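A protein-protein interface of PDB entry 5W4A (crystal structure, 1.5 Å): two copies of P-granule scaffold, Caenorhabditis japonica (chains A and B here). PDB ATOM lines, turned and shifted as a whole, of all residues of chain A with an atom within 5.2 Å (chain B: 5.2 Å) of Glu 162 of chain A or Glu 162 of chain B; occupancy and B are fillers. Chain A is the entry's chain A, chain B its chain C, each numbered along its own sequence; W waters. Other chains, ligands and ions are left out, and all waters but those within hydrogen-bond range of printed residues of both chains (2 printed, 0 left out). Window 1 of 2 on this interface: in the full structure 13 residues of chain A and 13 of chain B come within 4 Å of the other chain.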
ATOM      1  N   LYS A 131      19.753 -25.319  28.488  1.00  0.00           N
ATOM      2  CA  LYS A 131      20.828 -25.640  27.566  1.00  0.00           C
ATOM      3  C   LYS A 131      21.621 -24.391  27.192  1.00  0.00           C
ATOM      4  O   LYS A 131      22.831 -24.473  26.954  1.00  0.00           O
ATOM      5  CB  LYS A 131      20.279 -26.307  26.314  1.00  0.00           C
ATOM      6  CG  LYS A 131      21.347 -26.823  25.407  1.00  0.00           C
ATOM      7  CD  LYS A 131      20.788 -27.792  24.354  1.00  0.00           C
ATOM      8  CE  LYS A 131      21.925 -28.434  23.554  1.00  0.00           C
ATOM      9  NZ  LYS A 131      21.391 -29.391  22.522  1.00  0.00           N
ATOM     10  N   ILE A 143      19.869 -32.139  28.594  1.00  0.00           N
ATOM     11  CA  ILE A 143      19.930 -33.427  27.902  1.00  0.00           C
ATOM     12  C   ILE A 143      19.004 -34.433  28.564  1.00  0.00           C
ATOM     13  O   ILE A 143      18.293 -35.185  27.894  1.00  0.00           O
ATOM     14  CB  ILE A 143      21.375 -33.939  27.867  1.00  0.00           C
ATOM     15  CG1 ILE A 143      22.215 -33.058  26.951  1.00  0.00           C
ATOM     16  CG2 ILE A 143      21.417 -35.412  27.395  1.00  0.00           C
ATOM     17  CD1 ILE A 143      23.713 -33.161  27.170  1.00  0.00           C
ATOM     18  N   THR A 158      19.369 -39.672  19.510  1.00  0.00           N
ATOM     19  CA  THR A 158      19.795 -38.347  19.066  1.00  0.00           C
ATOM     20  C   THR A 158      20.011 -37.413  20.249  1.00  0.00           C
ATOM     21  O   THR A 158      21.023 -36.696  20.308  1.00  0.00           O
ATOM     22  CB  THR A 158      18.760 -37.776  18.095  1.00  0.00           C
ATOM     23  OG1 THR A 158      18.599 -38.654  16.964  1.00  0.00           O
ATOM     24  CG2 THR A 158      19.171 -36.400  17.592  1.00  0.00           C
ATOM     25  N   GLU A 159      19.107 -37.449  21.223  1.00  0.00           N
ATOM     26  CA  GLU A 159      19.246 -36.540  22.356  1.00  0.00           C
ATOM     27  C   GLU A 159      20.360 -36.993  23.285  1.00  0.00           C
ATOM     28  O   GLU A 159      21.163 -36.163  23.746  1.00  0.00           O
ATOM     29  CB  GLU A 159      17.923 -36.394  23.101  1.00  0.00           C
ATOM     30  CG  GLU A 159      16.791 -35.783  22.268  1.00  0.00           C
ATOM     31  CD  GLU A 159      17.085 -34.380  21.714  1.00  0.00           C
ATOM     32  OE1 GLU A 159      18.019 -33.667  22.140  1.00  0.00           O
ATOM     33  OE2 GLU A 159      16.328 -33.954  20.806  1.00  0.00           O
ATOM     34  N   LEU A 160      20.468 -38.293  23.539  1.00  0.00           N
ATOM     35  CA  LEU A 160      21.577 -38.773  24.368  1.00  0.00           C
ATOM     36  C   LEU A 160      22.943 -38.535  23.721  1.00  0.00           C
ATOM     37  O   LEU A 160      23.951 -38.352  24.432  1.00  0.00           O
ATOM     38  CB  LEU A 160      21.379 -40.256  24.681  1.00  0.00           C
ATOM     39  CG  LEU A 160      20.308 -40.524  25.720  1.00  0.00           C
ATOM     40  CD1 LEU A 160      19.924 -42.006  25.667  1.00  0.00           C
ATOM     41  CD2 LEU A 160      20.749 -40.100  27.100  1.00  0.00           C
ATOM     42  N   SER A 161      23.019 -38.523  22.386  1.00  0.00           N
ATOM     43  CA  SER A 161      24.269 -38.229  21.697  1.00  0.00           C
ATOM     44  C   SER A 161      24.856 -36.890  22.122  1.00  0.00           C
ATOM     45  O   SER A 161      26.072 -36.700  22.039  1.00  0.00           O
ATOM     46  CB  SER A 161      24.057 -38.250  20.182  1.00  0.00           C
ATOM     47  OG  SER A 161      23.884 -39.594  19.728  1.00  0.00           O
ATOM     48  N   GLU A 162      24.000 -35.950  22.526  1.00  0.00           N
ATOM     49  CA  GLU A 162      24.467 -34.634  22.967  1.00  0.00           C
ATOM     50  C   GLU A 162      25.382 -34.739  24.176  1.00  0.00           C
ATOM     51  O   GLU A 162      26.191 -33.831  24.399  1.00  0.00           O
ATOM     52  CB  GLU A 162      23.296 -33.687  23.284  1.00  0.00           C
ATOM     53  CG  GLU A 162      22.477 -33.324  22.055  1.00  0.00           C
ATOM     54  CD  GLU A 162      23.266 -32.483  21.067  1.00  0.00           C
ATOM     55  OE1 GLU A 162      23.976 -31.560  21.521  1.00  0.00           O
ATOM     56  OE2 GLU A 162      23.238 -32.779  19.851  1.00  0.00           O
ATOM     57  N   LEU A 163      25.322 -35.847  24.925  1.00  0.00           N
ATOM     58  CA  LEU A 163      26.298 -36.059  26.000  1.00  0.00           C
ATOM     59  C   LEU A 163      27.732 -35.998  25.504  1.00  0.00           C
ATOM     60  O   LEU A 163      28.639 -35.615  26.261  1.00  0.00           O
ATOM     61  CB  LEU A 163      26.049 -37.413  26.670  1.00  0.00           C
ATOM     62  CG  LEU A 163      24.763 -37.454  27.489  1.00  0.00           C
ATOM     63  CD1 LEU A 163      24.391 -38.897  27.849  1.00  0.00           C
ATOM     64  CD2 LEU A 163      24.809 -36.604  28.769  1.00  0.00           C
ATOM     65  N   CYS A 164      27.979 -36.394  24.253  1.00  0.00           N
ATOM     66  CA  CYS A 164      29.325 -36.352  23.714  1.00  0.00           C
ATOM     67  C   CYS A 164      29.871 -34.930  23.667  1.00  0.00           C
ATOM     68  O   CYS A 164      31.084 -34.741  23.708  1.00  0.00           O
ATOM     69  CB  CYS A 164      29.380 -37.004  22.329  1.00  0.00           C
ATOM     70  SG  CYS A 164      28.822 -38.759  22.389  1.00  0.00           S
ATOM     71  N   GLY A 165      28.998 -33.929  23.578  1.00  0.00           N
ATOM     72  CA  GLY A 165      29.438 -32.546  23.594  1.00  0.00           C
ATOM     73  C   GLY A 165      30.005 -32.098  24.918  1.00  0.00           C
ATOM     74  O   GLY A 165      30.659 -31.049  24.969  1.00  0.00           O
ATOM     75  N   LEU A 166      29.769 -32.864  25.970  1.00  0.00           N
ATOM     76  CA  LEU A 166      30.358 -32.673  27.293  1.00  0.00           C
ATOM     77  C   LEU A 166      31.439 -33.701  27.577  1.00  0.00           C
ATOM     78  O   LEU A 166      31.831 -33.878  28.736  1.00  0.00           O
ATOM     79  CB  LEU A 166      29.269 -32.774  28.358  1.00  0.00           C
ATOM     80  CG  LEU A 166      28.051 -31.847  28.205  1.00  0.00           C
ATOM     81  CD1 LEU A 166      26.942 -32.152  29.217  1.00  0.00           C
ATOM     82  CD2 LEU A 166      28.499 -30.409  28.320  1.00  0.00           C
ATOM     83  N   LYS B 131      29.034 -33.683  14.277  1.00  0.00           N
ATOM     84  CA  LYS B 131      28.811 -33.145  15.609  1.00  0.00           C
ATOM     85  C   LYS B 131      29.512 -33.974  16.675  1.00  0.00           C
ATOM     86  O   LYS B 131      29.904 -33.437  17.709  1.00  0.00           O
ATOM     87  CB  LYS B 131      27.324 -33.036  15.893  1.00  0.00           C
ATOM     88  CG  LYS B 131      27.013 -32.239  17.131  1.00  0.00           C
ATOM     89  CD  LYS B 131      25.546 -31.924  17.237  1.00  0.00           C
ATOM     90  CE  LYS B 131      25.344 -30.948  18.376  1.00  0.00           C
ATOM     91  NZ  LYS B 131      23.938 -30.561  18.513  1.00  0.00           N
ATOM     92  N   ILE B 143      26.148 -27.776  12.798  1.00  0.00           N
ATOM     93  CA  ILE B 143      25.101 -26.786  13.047  1.00  0.00           C
ATOM     94  C   ILE B 143      24.643 -26.158  11.733  1.00  0.00           C
ATOM     95  O   ILE B 143      23.441 -25.930  11.522  1.00  0.00           O
ATOM     96  CB  ILE B 143      25.586 -25.732  14.058  1.00  0.00           C
ATOM     97  CG1 ILE B 143      25.724 -26.370  15.424  1.00  0.00           C
ATOM     98  CG2 ILE B 143      24.604 -24.525  14.124  1.00  0.00           C
ATOM     99  CD1 ILE B 143      26.586 -25.528  16.373  1.00  0.00           C
ATOM    100  N   THR B 158      15.845 -23.319  16.726  1.00  0.00           N
ATOM    101  CA  THR B 158      16.324 -24.362  17.626  1.00  0.00           C
ATOM    102  C   THR B 158      17.714 -24.841  17.227  1.00  0.00           C
ATOM    103  O   THR B 158      18.592 -25.018  18.091  1.00  0.00           O
ATOM    104  CB  THR B 158      15.325 -25.533  17.623  1.00  0.00           C
ATOM    105  OG1 THR B 158      14.054 -25.064  18.094  1.00  0.00           O
ATOM    106  CG2 THR B 158      15.786 -26.666  18.494  1.00  0.00           C
ATOM    107  N   GLU B 159      17.939 -25.049  15.938  1.00  0.00           N
ATOM    108  CA  GLU B 159      19.241 -25.551  15.493  1.00  0.00           C
ATOM    109  C   GLU B 159      20.320 -24.462  15.580  1.00  0.00           C
ATOM    110  O   GLU B 159      21.438 -24.727  16.039  1.00  0.00           O
ATOM    111  CB  GLU B 159      19.150 -26.122  14.074  1.00  0.00           C
ATOM    112  CG  GLU B 159      18.216 -27.336  13.970  1.00  0.00           C
ATOM    113  CD  GLU B 159      18.651 -28.558  14.808  1.00  0.00           C
ATOM    114  OE1 GLU B 159      19.771 -28.614  15.340  1.00  0.00           O
ATOM    115  OE2 GLU B 159      17.825 -29.503  14.909  1.00  0.00           O
ATOM    116  N   LEU B 160      20.001 -23.230  15.183  1.00  0.00           N
ATOM    117  CA  LEU B 160      20.965 -22.133  15.329  1.00  0.00           C
ATOM    118  C   LEU B 160      21.324 -21.882  16.791  1.00  0.00           C
ATOM    119  O   LEU B 160      22.428 -21.410  17.106  1.00  0.00           O
ATOM    120  CB  LEU B 160      20.391 -20.865  14.709  1.00  0.00           C
ATOM    121  CG  LEU B 160      20.383 -20.808  13.195  1.00  0.00           C
ATOM    122  CD1 LEU B 160      19.479 -19.707  12.669  1.00  0.00           C
ATOM    123  CD2 LEU B 160      21.812 -20.627  12.677  1.00  0.00           C
ATOM    124  N   SER B 161      20.392 -22.137  17.707  1.00  0.00           N
ATOM    125  CA  SER B 161      20.661 -21.953  19.126  1.00  0.00           C
ATOM    126  C   SER B 161      21.839 -22.805  19.584  1.00  0.00           C
ATOM    127  O   SER B 161      22.504 -22.450  20.561  1.00  0.00           O
ATOM    128  CB  SER B 161      19.424 -22.307  19.959  1.00  0.00           C
ATOM    129  OG  SER B 161      18.399 -21.309  19.849  1.00  0.00           O
ATOM    130  N   GLU B 162      22.128 -23.905  18.873  1.00  0.00           N
ATOM    131  CA  GLU B 162      23.270 -24.740  19.238  1.00  0.00           C
ATOM    132  C   GLU B 162      24.584 -23.974  19.113  1.00  0.00           C
ATOM    133  O   GLU B 162      25.583 -24.372  19.729  1.00  0.00           O
ATOM    134  CB  GLU B 162      23.316 -26.007  18.357  1.00  0.00           C
ATOM    135  CG  GLU B 162      22.168 -26.982  18.614  1.00  0.00           C
ATOM    136  CD  GLU B 162      22.228 -27.608  19.983  1.00  0.00           C
ATOM    137  OE1 GLU B 162      23.342 -27.992  20.436  1.00  0.00           O
ATOM    138  OE2 GLU B 162      21.167 -27.636  20.641  1.00  0.00           O
ATOM    139  N   LEU B 163      24.597 -22.852  18.371  1.00  0.00           N
ATOM    140  CA  LEU B 163      25.810 -22.019  18.325  1.00  0.00           C
ATOM    141  C   LEU B 163      26.223 -21.546  19.712  1.00  0.00           C
ATOM    142  O   LEU B 163      27.413 -21.340  19.970  1.00  0.00           O
ATOM    143  CB  LEU B 163      25.585 -20.816  17.394  1.00  0.00           C
ATOM    144  CG  LEU B 163      25.484 -21.203  15.939  1.00  0.00           C
ATOM    145  CD1 LEU B 163      24.922 -20.023  15.126  1.00  0.00           C
ATOM    146  CD2 LEU B 163      26.849 -21.659  15.355  1.00  0.00           C
ATOM    147  N   CYS B 164      25.257 -21.354  20.624  1.00  0.00           N
ATOM    148  CA  CYS B 164      25.559 -20.910  21.973  1.00  0.00           C
ATOM    149  C   CYS B 164      26.407 -21.931  22.719  1.00  0.00           C
ATOM    150  O   CYS B 164      27.146 -21.546  23.617  1.00  0.00           O
ATOM    151  CB  CYS B 164      24.273 -20.623  22.734  1.00  0.00           C
ATOM    152  SG  CYS B 164      23.262 -19.325  21.938  1.00  0.00           S
ATOM    153  N   GLY B 165      26.373 -23.208  22.305  1.00  0.00           N
ATOM    154  CA  GLY B 165      27.219 -24.220  22.912  1.00  0.00           C
ATOM    155  C   GLY B 165      28.677 -24.107  22.547  1.00  0.00           C
ATOM    156  O   GLY B 165      29.507 -24.770  23.182  1.00  0.00           O
ATOM    157  N   LEU B 166      28.995 -23.344  21.492  1.00  0.00           N
ATOM    158  CA  LEU B 166      30.357 -22.969  21.117  1.00  0.00           C
ATOM    159  C   LEU B 166      30.693 -21.531  21.519  1.00  0.00           C
ATOM    160  O   LEU B 166      31.688 -20.961  21.045  1.00  0.00           O
ATOM    161  CB  LEU B 166      30.537 -23.155  19.610  1.00  0.00           C
ATOM    162  CG  LEU B 166      30.271 -24.552  19.051  1.00  0.00           C
ATOM    163  CD1 LEU B 166      30.228 -24.549  17.529  1.00  0.00           C
ATOM    164  CD2 LEU B 166      31.368 -25.469  19.552  1.00  0.00           C
HETATM  165  O   HOH W   1      29.799 -34.069  20.369  1.00  0.00           O
HETATM  166  O   HOH W   2      24.366 -23.388  24.948  1.00  0.00           O
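The side-chain carboxylate of Glu 162 of chain A is in salt-bridge range of the side-chain amino group of Lys 131 of chain B, 2.7 Å away. OE2 of Glu 162 of chain B is in salt-bridge range of NZ of Lys 131 of chain A (2.6 Å).
The side-chain amino group (NZ) of Lys 131 of chain A lies within salt-bridge range of the side-chain carboxylate (OE1) of Glu 162 of chain A. The side-chain amino group of Lys 131 of chain B lies within salt-bridge range of the side-chain carboxylate of Glu 162 of chain B, at 3.3 Å.
Among the printed residues, merely in contact across the chains: Glu 162 of chain A with Glu 162 of chain B (3.8 Å).
Printed residues of chain B within 4 Å of Lys 131 of chain A: Glu 162. Glu 162 of chain A touches two residues of chain B. Of the printed residues of chain A, Lys 131 of chain B touches Glu 162 (2.7 Å). Printed residues of chain A within 4 Å of Glu 162 of chain B: Lys 131 (2.6 Å) and Glu 162 (3.8 Å). The nearest printed residue of chain B that does not touch Glu 162 of chain A is Glu 159 of chain B (7.1 Å). The nearest printed residue of chain B that does not touch Lys 131 of chain A is Lys 131 of chain B (4.9 Å).
Of the 11 printed residues of chain B, 2 touch a printed residue of chain A. Printed residues of chain B that touch a printed residue of chain A: Lys 131 and Glu 162. Printed residues of chain A that touch a printed residue of chain B: Lys 131 and Glu 162. Among the printed residues, 3 pairs touch across the chains. Among the printed residues, Asp or Glu carboxylates within 4 Å of a Lys or Arg side-chain nitrogen of the other chain: Lys 131 of chain A with Glu 162 of chain B and Glu 162 of chain A with Lys 131 of chain B.
Lys 131 of chain A touches Glu 162 of chain B, and with the chains exchanged Glu 162 of chain A touches Lys 131 of chain B. Glu 162 of chain A touches its own counterpart, Glu 162 of chain B. Positions printed for both chains: 131, 143, 158, 159, 160, 161, 162, 163, 164, 165 and 166. Of the 3 pairs that touch across the chains among the printed residues, 3 have their exchanged pair printed and touching as well.
Water W1 bridges O of Lys 131 of chain B and N of Gly 165 of chain A. Water W2 lies within hydrogen-bond range of the backbone carbonyl oxygen of Lys 131 of chain A and the backbone NH of Gly 165 of chain B.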
